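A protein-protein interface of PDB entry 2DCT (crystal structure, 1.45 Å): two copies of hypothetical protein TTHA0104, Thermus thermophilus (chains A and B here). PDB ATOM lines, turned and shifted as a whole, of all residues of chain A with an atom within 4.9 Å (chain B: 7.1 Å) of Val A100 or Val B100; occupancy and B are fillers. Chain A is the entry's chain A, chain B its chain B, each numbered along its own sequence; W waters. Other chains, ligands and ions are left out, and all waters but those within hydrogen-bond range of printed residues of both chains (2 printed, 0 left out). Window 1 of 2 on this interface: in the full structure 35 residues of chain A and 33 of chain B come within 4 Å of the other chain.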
ATOM      1  N   MET A  28      11.592  -2.616  23.418  1.00  0.00           N
ATOM      2  CA  MET A  28      11.900  -3.630  24.391  1.00  0.00           C
ATOM      3  C   MET A  28      13.323  -4.074  24.259  1.00  0.00           C
ATOM      4  O   MET A  28      13.993  -3.789  23.272  1.00  0.00           O
ATOM      5  CB  MET A  28      11.011  -4.853  24.148  1.00  0.00           C
ATOM      6  CG  MET A  28      11.290  -5.527  22.803  1.00  0.00           C
ATOM      7  SD  MET A  28      10.297  -7.002  22.512  1.00  0.00           S
ATOM      8  CE  MET A  28       9.340  -6.518  21.086  1.00  0.00           C
ATOM      9  N   LEU A  29      13.779  -4.767  25.285  1.00  0.00           N
ATOM     10  CA  LEU A  29      15.084  -5.364  25.244  1.00  0.00           C
ATOM     11  C   LEU A  29      14.683  -6.789  24.940  1.00  0.00           C
ATOM     12  O   LEU A  29      13.720  -7.312  25.499  1.00  0.00           O
ATOM     13  CB  LEU A  29      15.780  -5.309  26.598  1.00  0.00           C
ATOM     14  CG  LEU A  29      16.167  -3.926  27.108  1.00  0.00           C
ATOM     15  CD1 LEU A  29      16.924  -4.093  28.407  1.00  0.00           C
ATOM     16  CD2 LEU A  29      17.025  -3.198  26.082  1.00  0.00           C
ATOM     17  N   TYR A  30      15.388  -7.404  24.016  1.00  0.00           N
ATOM     18  CA  TYR A  30      15.112  -8.777  23.656  1.00  0.00           C
ATOM     19  C   TYR A  30      16.542  -9.255  23.667  1.00  0.00           C
ATOM     20  O   TYR A  30      17.270  -9.120  22.685  1.00  0.00           O
ATOM     21  CB  TYR A  30      14.492  -8.834  22.266  1.00  0.00           C
ATOM     22  CG  TYR A  30      13.857 -10.160  21.929  1.00  0.00           C
ATOM     23  CD1 TYR A  30      12.495 -10.389  22.150  1.00  0.00           C
ATOM     24  CD2 TYR A  30      14.610 -11.181  21.363  1.00  0.00           C
ATOM     25  CE1 TYR A  30      11.907 -11.607  21.803  1.00  0.00           C
ATOM     26  CE2 TYR A  30      14.034 -12.394  21.014  1.00  0.00           C
ATOM     27  CZ  TYR A  30      12.685 -12.602  21.233  1.00  0.00           C
ATOM     28  OH  TYR A  30      12.122 -13.799  20.847  1.00  0.00           O
ATOM     29  N   ASP A  50       8.370  -4.530  32.411  1.00  0.00           N
ATOM     30  CA  ASP A  50       8.087  -5.910  32.740  1.00  0.00           C
ATOM     31  C   ASP A  50       9.208  -6.690  32.119  1.00  0.00           C
ATOM     32  O   ASP A  50       9.748  -6.306  31.086  1.00  0.00           O
ATOM     33  CB  ASP A  50       6.778  -6.378  32.126  1.00  0.00           C
ATOM     34  CG  ASP A  50       5.581  -5.879  32.874  1.00  0.00           C
ATOM     35  OD1 ASP A  50       5.759  -5.128  33.856  1.00  0.00           O
ATOM     36  OD2 ASP A  50       4.464  -6.244  32.476  1.00  0.00           O
ATOM     37  N   LYS A  51       9.553  -7.799  32.740  1.00  0.00           N
ATOM     38  CA  LYS A  51      10.623  -8.605  32.215  1.00  0.00           C
ATOM     39  C   LYS A  51      10.152 -10.032  32.220  1.00  0.00           C
ATOM     40  O   LYS A  51       9.450 -10.465  33.126  1.00  0.00           O
ATOM     41  CB  LYS A  51      11.862  -8.440  33.091  1.00  0.00           C
ATOM     42  CG  LYS A  51      13.133  -9.052  32.542  1.00  0.00           C
ATOM     43  CD  LYS A  51      14.335  -8.487  33.296  1.00  0.00           C
ATOM     44  CE  LYS A  51      15.645  -8.888  32.659  1.00  0.00           C
ATOM     45  NZ  LYS A  51      16.809  -8.242  33.324  1.00  0.00           N
ATOM     46  N   VAL A  52      10.495 -10.755  31.169  1.00  0.00           N
ATOM     47  CA  VAL A  52      10.133 -12.149  31.101  1.00  0.00           C
ATOM     48  C   VAL A  52      11.395 -12.898  30.755  1.00  0.00           C
ATOM     49  O   VAL A  52      12.107 -12.543  29.818  1.00  0.00           O
ATOM     50  CB  VAL A  52       9.070 -12.436  30.029  1.00  0.00           C
ATOM     51  CG1 VAL A  52       8.742 -13.915  30.027  1.00  0.00           C
ATOM     52  CG2 VAL A  52       7.816 -11.624  30.300  1.00  0.00           C
ATOM     53  N   LEU A  98      16.298 -16.217  27.181  1.00  0.00           N
ATOM     54  CA  LEU A  98      15.786 -15.250  26.231  1.00  0.00           C
ATOM     55  C   LEU A  98      15.092 -14.334  27.212  1.00  0.00           C
ATOM     56  O   LEU A  98      14.162 -14.749  27.907  1.00  0.00           O
ATOM     57  CB  LEU A  98      14.776 -15.881  25.283  1.00  0.00           C
ATOM     58  CG  LEU A  98      14.022 -14.876  24.413  1.00  0.00           C
ATOM     59  CD1 LEU A  98      14.986 -13.884  23.775  1.00  0.00           C
ATOM     60  CD2 LEU A  98      13.247 -15.642  23.356  1.00  0.00           C
ATOM     61  N   VAL A  99      15.555 -13.098  27.284  1.00  0.00           N
ATOM     62  CA  VAL A  99      15.015 -12.169  28.255  1.00  0.00           C
ATOM     63  C   VAL A  99      14.424 -10.956  27.588  1.00  0.00           C
ATOM     64  O   VAL A  99      15.101 -10.230  26.863  1.00  0.00           O
ATOM     65  CB  VAL A  99      16.122 -11.745  29.226  1.00  0.00           C
ATOM     66  CG1 VAL A  99      15.540 -10.930  30.345  1.00  0.00           C
ATOM     67  CG2 VAL A  99      16.829 -12.978  29.770  1.00  0.00           C
ATOM     68  N   VAL A 100      13.144 -10.744  27.841  1.00  0.00           N
ATOM     69  CA  VAL A 100      12.438  -9.633  27.254  1.00  0.00           C
ATOM     70  C   VAL A 100      12.107  -8.630  28.336  1.00  0.00           C
ATOM     71  O   VAL A 100      11.595  -8.993  29.390  1.00  0.00           O
ATOM     72  CB  VAL A 100      11.127 -10.106  26.606  1.00  0.00           C
ATOM     73  CG1 VAL A 100      10.380  -8.918  26.027  1.00  0.00           C
ATOM     74  CG2 VAL A 100      11.425 -11.138  25.525  1.00  0.00           C
ATOM     75  N   THR A 101      12.424  -7.371  28.079  1.00  0.00           N
ATOM     76  CA  THR A 101      12.114  -6.310  29.018  1.00  0.00           C
ATOM     77  C   THR A 101      11.381  -5.265  28.208  1.00  0.00           C
ATOM     78  O   THR A 101      11.864  -4.822  27.174  1.00  0.00           O
ATOM     79  CB  THR A 101      13.379  -5.682  29.627  1.00  0.00           C
ATOM     80  OG1 THR A 101      14.155  -6.702  30.262  1.00  0.00           O
ATOM     81  CG2 THR A 101      13.010  -4.639  30.670  1.00  0.00           C
ATOM     82  N   ALA A 102      10.199  -4.889  28.664  1.00  0.00           N
ATOM     83  CA  ALA A 102       9.432  -3.889  27.950  1.00  0.00           C
ATOM     84  C   ALA A 102       8.734  -2.998  28.946  1.00  0.00           C
ATOM     85  O   ALA A 102       8.159  -3.473  29.911  1.00  0.00           O
ATOM     86  CB  ALA A 102       8.407  -4.556  27.039  1.00  0.00           C
ATOM     87  N   MET B  28       3.386  -5.618  27.289  1.00  0.00           N
ATOM     88  CA  MET B  28       3.700  -6.420  26.127  1.00  0.00           C
ATOM     89  C   MET B  28       2.717  -7.553  26.025  1.00  0.00           C
ATOM     90  O   MET B  28       1.937  -7.805  26.936  1.00  0.00           O
ATOM     91  CB  MET B  28       5.092  -7.038  26.278  1.00  0.00           C
ATOM     92  CG  MET B  28       5.143  -8.097  27.375  1.00  0.00           C
ATOM     93  SD  MET B  28       6.729  -8.938  27.526  1.00  0.00           S
ATOM     94  CE  MET B  28       7.531  -7.916  28.750  1.00  0.00           C
ATOM     95  N   LEU B  29       2.761  -8.226  24.888  1.00  0.00           N
ATOM     96  CA  LEU B  29       1.976  -9.420  24.692  1.00  0.00           C
ATOM     97  C   LEU B  29       3.082 -10.449  24.644  1.00  0.00           C
ATOM     98  O   LEU B  29       4.113 -10.245  24.003  1.00  0.00           O
ATOM     99  CB  LEU B  29       1.225  -9.420  23.366  1.00  0.00           C
ATOM    100  CG  LEU B  29       0.121  -8.385  23.217  1.00  0.00           C
ATOM    101  CD1 LEU B  29      -0.659  -8.702  21.951  1.00  0.00           C
ATOM    102  CD2 LEU B  29      -0.802  -8.403  24.428  1.00  0.00           C
ATOM    103  N   TYR B  30       2.887 -11.536  25.358  1.00  0.00           N
ATOM    104  CA  TYR B  30       3.862 -12.599  25.394  1.00  0.00           C
ATOM    105  C   TYR B  30       2.958 -13.786  25.161  1.00  0.00           C
ATOM    106  O   TYR B  30       2.429 -14.384  26.094  1.00  0.00           O
ATOM    107  CB  TYR B  30       4.512 -12.635  26.770  1.00  0.00           C
ATOM    108  CG  TYR B  30       5.789 -13.420  26.826  1.00  0.00           C
ATOM    109  CD1 TYR B  30       7.021 -12.814  26.576  1.00  0.00           C
ATOM    110  CD2 TYR B  30       5.770 -14.769  27.155  1.00  0.00           C
ATOM    111  CE1 TYR B  30       8.201 -13.540  26.666  1.00  0.00           C
ATOM    112  CE2 TYR B  30       6.938 -15.498  27.246  1.00  0.00           C
ATOM    113  CZ  TYR B  30       8.148 -14.880  27.004  1.00  0.00           C
ATOM    114  OH  TYR B  30       9.299 -15.613  27.136  1.00  0.00           O
ATOM    115  N   ASP B  31       2.773 -14.096  23.886  1.00  0.00           N
ATOM    116  CA  ASP B  31       1.869 -15.152  23.472  1.00  0.00           C
ATOM    117  C   ASP B  31       2.517 -16.285  22.741  1.00  0.00           C
ATOM    118  O   ASP B  31       3.632 -16.185  22.248  1.00  0.00           O
ATOM    119  CB  ASP B  31       0.819 -14.621  22.492  1.00  0.00           C
ATOM    120  CG  ASP B  31      -0.039 -13.530  23.059  1.00  0.00           C
ATOM    121  OD1 ASP B  31      -0.064 -13.348  24.285  1.00  0.00           O
ATOM    122  OD2 ASP B  31      -0.716 -12.866  22.249  1.00  0.00           O
ATOM    123  N   TYR B  33       1.751 -18.722  19.511  1.00  0.00           N
ATOM    124  CA  TYR B  33       0.916 -18.793  18.327  1.00  0.00           C
ATOM    125  C   TYR B  33       0.999 -20.246  17.950  1.00  0.00           C
ATOM    126  O   TYR B  33       2.085 -20.759  17.695  1.00  0.00           O
ATOM    127  CB  TYR B  33       1.471 -17.954  17.189  1.00  0.00           C
ATOM    128  CG  TYR B  33       1.114 -16.501  17.270  1.00  0.00           C
ATOM    129  CD1 TYR B  33       0.777 -15.908  18.485  1.00  0.00           C
ATOM    130  CD2 TYR B  33       1.173 -15.698  16.139  1.00  0.00           C
ATOM    131  CE1 TYR B  33       0.513 -14.548  18.567  1.00  0.00           C
ATOM    132  CE2 TYR B  33       0.913 -14.343  16.211  1.00  0.00           C
ATOM    133  CZ  TYR B  33       0.586 -13.773  17.425  1.00  0.00           C
ATOM    134  OH  TYR B  33       0.344 -12.423  17.488  1.00  0.00           O
ATOM    135  N   ASP B  50       6.240  -3.377  18.248  1.00  0.00           N
ATOM    136  CA  ASP B  50       7.296  -4.187  17.682  1.00  0.00           C
ATOM    137  C   ASP B  50       6.912  -5.597  18.044  1.00  0.00           C
ATOM    138  O   ASP B  50       6.395  -5.843  19.129  1.00  0.00           O
ATOM    139  CB  ASP B  50       8.632  -3.876  18.341  1.00  0.00           C
ATOM    140  CG  ASP B  50       9.281  -2.643  17.787  1.00  0.00           C
ATOM    141  OD1 ASP B  50       8.619  -1.901  17.034  1.00  0.00           O
ATOM    142  OD2 ASP B  50      10.459  -2.415  18.112  1.00  0.00           O
ATOM    143  N   LYS B  51       7.151  -6.525  17.137  1.00  0.00           N
ATOM    144  CA  LYS B  51       6.836  -7.904  17.420  1.00  0.00           C
ATOM    145  C   LYS B  51       8.054  -8.740  17.114  1.00  0.00           C
ATOM    146  O   LYS B  51       8.834  -8.430  16.217  1.00  0.00           O
ATOM    147  CB  LYS B  51       5.650  -8.374  16.565  1.00  0.00           C
ATOM    148  CG  LYS B  51       5.298  -9.846  16.736  1.00  0.00           C
ATOM    149  CD  LYS B  51       3.994 -10.210  16.027  1.00  0.00           C
ATOM    150  CE  LYS B  51       2.781  -9.676  16.770  1.00  0.00           C
ATOM    151  NZ  LYS B  51       1.503 -10.044  16.096  1.00  0.00           N
ATOM    152  N   VAL B  52       8.251  -9.778  17.904  1.00  0.00           N
ATOM    153  CA  VAL B  52       9.342 -10.681  17.650  1.00  0.00           C
ATOM    154  C   VAL B  52       8.719 -12.057  17.670  1.00  0.00           C
ATOM    155  O   VAL B  52       8.012 -12.418  18.613  1.00  0.00           O
ATOM    156  CB  VAL B  52      10.447 -10.610  18.717  1.00  0.00           C
ATOM    157  CG1 VAL B  52      11.512 -11.654  18.410  1.00  0.00           C
ATOM    158  CG2 VAL B  52      11.079  -9.226  18.728  1.00  0.00           C
ATOM    159  N   TYR B  53       8.945 -12.804  16.600  1.00  0.00           N
ATOM    160  CA  TYR B  53       8.438 -14.157  16.507  1.00  0.00           C
ATOM    161  C   TYR B  53       9.612 -15.043  16.822  1.00  0.00           C
ATOM    162  O   TYR B  53      10.700 -14.852  16.285  1.00  0.00           O
ATOM    163  CB  TYR B  53       7.991 -14.494  15.095  1.00  0.00           C
ATOM    164  CG  TYR B  53       6.797 -13.739  14.594  1.00  0.00           C
ATOM    165  CD1 TYR B  53       5.507 -14.133  14.935  1.00  0.00           C
ATOM    166  CD2 TYR B  53       6.951 -12.663  13.730  1.00  0.00           C
ATOM    167  CE1 TYR B  53       4.400 -13.479  14.420  1.00  0.00           C
ATOM    168  CE2 TYR B  53       5.852 -12.001  13.210  1.00  0.00           C
ATOM    169  CZ  TYR B  53       4.580 -12.416  13.555  1.00  0.00           C
ATOM    170  OH  TYR B  53       3.491 -11.779  13.013  1.00  0.00           O
ATOM    171  N   TYR B  54       9.398 -16.004  17.697  1.00  0.00           N
ATOM    172  CA  TYR B  54      10.448 -16.935  18.033  1.00  0.00           C
ATOM    173  C   TYR B  54       9.833 -18.308  17.850  1.00  0.00           C
ATOM    174  O   TYR B  54       8.767 -18.597  18.390  1.00  0.00           O
ATOM    175  CB  TYR B  54      10.908 -16.733  19.473  1.00  0.00           C
ATOM    176  CG  TYR B  54      11.853 -17.806  19.931  1.00  0.00           C
ATOM    177  CD1 TYR B  54      13.152 -17.879  19.427  1.00  0.00           C
ATOM    178  CD2 TYR B  54      11.441 -18.772  20.838  1.00  0.00           C
ATOM    179  CE1 TYR B  54      14.011 -18.893  19.819  1.00  0.00           C
ATOM    180  CE2 TYR B  54      12.289 -19.790  21.233  1.00  0.00           C
ATOM    181  CZ  TYR B  54      13.571 -19.843  20.720  1.00  0.00           C
ATOM    182  OH  TYR B  54      14.407 -20.861  21.105  1.00  0.00           O
ATOM    183  N   ALA B  77      12.541 -13.693  14.690  1.00  0.00           N
ATOM    184  CA  ALA B  77      12.470 -12.704  13.634  1.00  0.00           C
ATOM    185  C   ALA B  77      11.837 -11.472  14.238  1.00  0.00           C
ATOM    186  O   ALA B  77      10.822 -11.548  14.929  1.00  0.00           O
ATOM    187  CB  ALA B  77      11.636 -13.216  12.477  1.00  0.00           C
ATOM    188  N   ALA B  79       9.946  -7.962  13.885  1.00  0.00           N
ATOM    189  CA  ALA B  79       9.032  -7.224  13.027  1.00  0.00           C
ATOM    190  C   ALA B  79       8.808  -5.892  13.717  1.00  0.00           C
ATOM    191  O   ALA B  79       7.876  -5.735  14.501  1.00  0.00           O
ATOM    192  CB  ALA B  79       7.712  -7.973  12.881  1.00  0.00           C
ATOM    193  N   LEU B  97       4.926 -20.765  18.092  1.00  0.00           N
ATOM    194  CA  LEU B  97       5.785 -19.608  18.196  1.00  0.00           C
ATOM    195  C   LEU B  97       5.584 -18.876  19.495  1.00  0.00           C
ATOM    196  O   LEU B  97       4.490 -18.882  20.055  1.00  0.00           O
ATOM    197  CB  LEU B  97       5.474 -18.623  17.078  1.00  0.00           C
ATOM    198  CG  LEU B  97       5.302 -19.189  15.678  1.00  0.00           C
ATOM    199  CD1 LEU B  97       4.945 -18.055  14.741  1.00  0.00           C
ATOM    200  CD2 LEU B  97       6.582 -19.874  15.232  1.00  0.00           C
ATOM    201  N   LEU B  98       6.659 -18.268  19.975  1.00  0.00           N
ATOM    202  CA  LEU B  98       6.601 -17.421  21.146  1.00  0.00           C
ATOM    203  C   LEU B  98       6.610 -16.078  20.449  1.00  0.00           C
ATOM    204  O   LEU B  98       7.574 -15.732  19.761  1.00  0.00           O
ATOM    205  CB  LEU B  98       7.847 -17.553  22.012  1.00  0.00           C
ATOM    206  CG  LEU B  98       7.964 -16.423  23.040  1.00  0.00           C
ATOM    207  CD1 LEU B  98       6.712 -16.372  23.905  1.00  0.00           C
ATOM    208  CD2 LEU B  98       9.198 -16.635  23.891  1.00  0.00           C
ATOM    209  N   VAL B  99       5.528 -15.335  20.595  1.00  0.00           N
ATOM    210  CA  VAL B  99       5.415 -14.058  19.936  1.00  0.00           C
ATOM    211  C   VAL B  99       5.319 -12.979  20.979  1.00  0.00           C
ATOM    212  O   VAL B  99       4.439 -13.003  21.835  1.00  0.00           O
ATOM    213  CB  VAL B  99       4.181 -14.041  19.024  1.00  0.00           C
ATOM    214  CG1 VAL B  99       4.154 -12.772  18.206  1.00  0.00           C
ATOM    215  CG2 VAL B  99       4.209 -15.258  18.110  1.00  0.00           C
ATOM    216  N   VAL B 100       6.254 -12.043  20.911  1.00  0.00           N
ATOM    217  CA  VAL B 100       6.306 -10.945  21.853  1.00  0.00           C
ATOM    218  C   VAL B 100       5.996  -9.669  21.119  1.00  0.00           C
ATOM    219  O   VAL B 100       6.558  -9.390  20.065  1.00  0.00           O
ATOM    220  CB  VAL B 100       7.698 -10.838  22.491  1.00  0.00           C
ATOM    221  CG1 VAL B 100       7.771  -9.619  23.390  1.00  0.00           C
ATOM    222  CG2 VAL B 100       7.998 -12.099  23.273  1.00  0.00           C
ATOM    223  N   THR B 101       5.078  -8.905  21.679  1.00  0.00           N
ATOM    224  CA  THR B 101       4.682  -7.649  21.098  1.00  0.00           C
ATOM    225  C   THR B 101       4.874  -6.611  22.177  1.00  0.00           C
ATOM    226  O   THR B 101       4.457  -6.809  23.308  1.00  0.00           O
ATOM    227  CB  THR B 101       3.207  -7.677  20.686  1.00  0.00           C
ATOM    228  OG1 THR B 101       2.999  -8.737  19.750  1.00  0.00           O
ATOM    229  CG2 THR B 101       2.809  -6.362  20.055  1.00  0.00           C
ATOM    230  N   ALA B 102       5.544  -5.520  21.838  1.00  0.00           N
ATOM    231  CA  ALA B 102       5.755  -4.446  22.787  1.00  0.00           C
ATOM    232  C   ALA B 102       5.613  -3.152  22.013  1.00  0.00           C
ATOM    233  O   ALA B 102       6.136  -3.021  20.920  1.00  0.00           O
ATOM    234  CB  ALA B 102       7.140  -4.539  23.413  1.00  0.00           C
ATOM    235  N   PRO B 103       4.866  -2.193  22.560  1.00  0.00           N
ATOM    236  CA  PRO B 103       4.184  -2.317  23.844  1.00  0.00           C
ATOM    237  C   PRO B 103       2.936  -3.154  23.635  1.00  0.00           C
ATOM    238  O   PRO B 103       2.732  -3.745  22.574  1.00  0.00           O
ATOM    239  CB  PRO B 103       3.830  -0.869  24.200  1.00  0.00           C
ATOM    240  CG  PRO B 103       3.747  -0.118  22.885  1.00  0.00           C
ATOM    241  CD  PRO B 103       4.740  -0.830  22.026  1.00  0.00           C
HETATM  242  O   HOH W   1       9.408 -13.744  20.511  1.00  0.00           O
HETATM  243  O   HOH W   2      11.534 -14.054  27.605  1.00  0.00           O
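Of the printed residues of chain B, Tyr A30 touches Val B52 (3.2 Å) and Tyr B54 (3.5 Å).
Leu A98 touches none of the printed residues of chain B.
Val A100 touches two residues of chain B.
Printed residues of chain A within 4 Å of Tyr B30: Val A52 (3.2 Å).
Of the printed residues of chain A, Tyr B54 touches Tyr A30 (3.5 Å).
Ala B79 touches none of the printed residues of chain A.
Val B100 touches two residues of chain A.
Of the printed residues of chain A, Ala B102 touches Met A28 and Ala A102.
The nearest printed residue of chain A that does not touch Tyr B30 is Val A100 (4.2 Å).
Asp B50 touches Met A28 (O to CE, 3.6 Å).
Val B100 touches Met A28 (CG1 to SD, 3.7 Å).
Met A28 touches Ala B102 (CE to CB, 3.8 Å).
Tyr A30 touches Val B52 (CZ to CG1, 3.2 Å).
Tyr B54 touches Tyr A30.
Met B28 touches Asp A50.
Val A52 touches Tyr B30 (CG1 to CZ, 3.2 Å).
Val A100 touches Met B28.
Val A100 touches Val B100.
Ala B102 touches Ala A102 (CB to CB, 3.8 Å).
Hydrophobic or aromatic side chains of chain B that line the printed part of chain A: Met B28, Tyr B30, Val B52, Tyr B54, Val B100 and Ala B102.
Of the 11 printed residues of chain A, 6 touch a printed residue of chain B.
Hydrophobic or aromatic side chains of chain A that line the printed part of chain B: Met A28, Tyr A30, Val A52, Val A100 and Ala A102.
Among the printed residues, 12 pairs touch across the chains.
Among the printed residues, no Asp or Glu carboxylate lies within 4 Å of a Lys or Arg side-chain nitrogen of the other chain.
N of Leu B98 is in hydrogen-bond range of O of Tyr B54, at 2.7 Å.
N of Val B52 sits at hydrogen-bond distance from O of Val B100, at 2.8 Å.
The backbone carbonyl oxygen (O) of Ala A102 lies within hydrogen-bond range of the backbone NH (N) of Asp A50 (2.7 Å).
O of Val A100 is in hydrogen-bond range of N of Val A52.
The backbone NH (N) of Asp B50 lies within hydrogen-bond range of the backbone carbonyl oxygen (O) of Ala B102 (2.7 Å).
Water W1 lies within hydrogen-bond range of the backbone carbonyl oxygen of Val B52, the side-chain hydroxyl of Tyr A30 and the backbone carbonyl oxygen of Leu B98.
Water W2 lies within hydrogen-bond range of O of Leu A98, O of Val A52 and OH of Tyr B30.
Met A28 touches Asp B50, and with the chains exchanged Asp A50 touches Met B28.
Met A28 touches Val B52, but with the chains exchanged Val A52 does not touch Met B28 (4.01 Å).
Met A28 touches Val B100, and with the chains exchanged Val A100 touches Met B28.
Met A28 touches Ala B102, and with the chains exchanged Ala A102 touches Met B28.
Of the 12 pairs that touch across the chains among the printed residues, 10 have their exchanged pair printed and touching as well.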
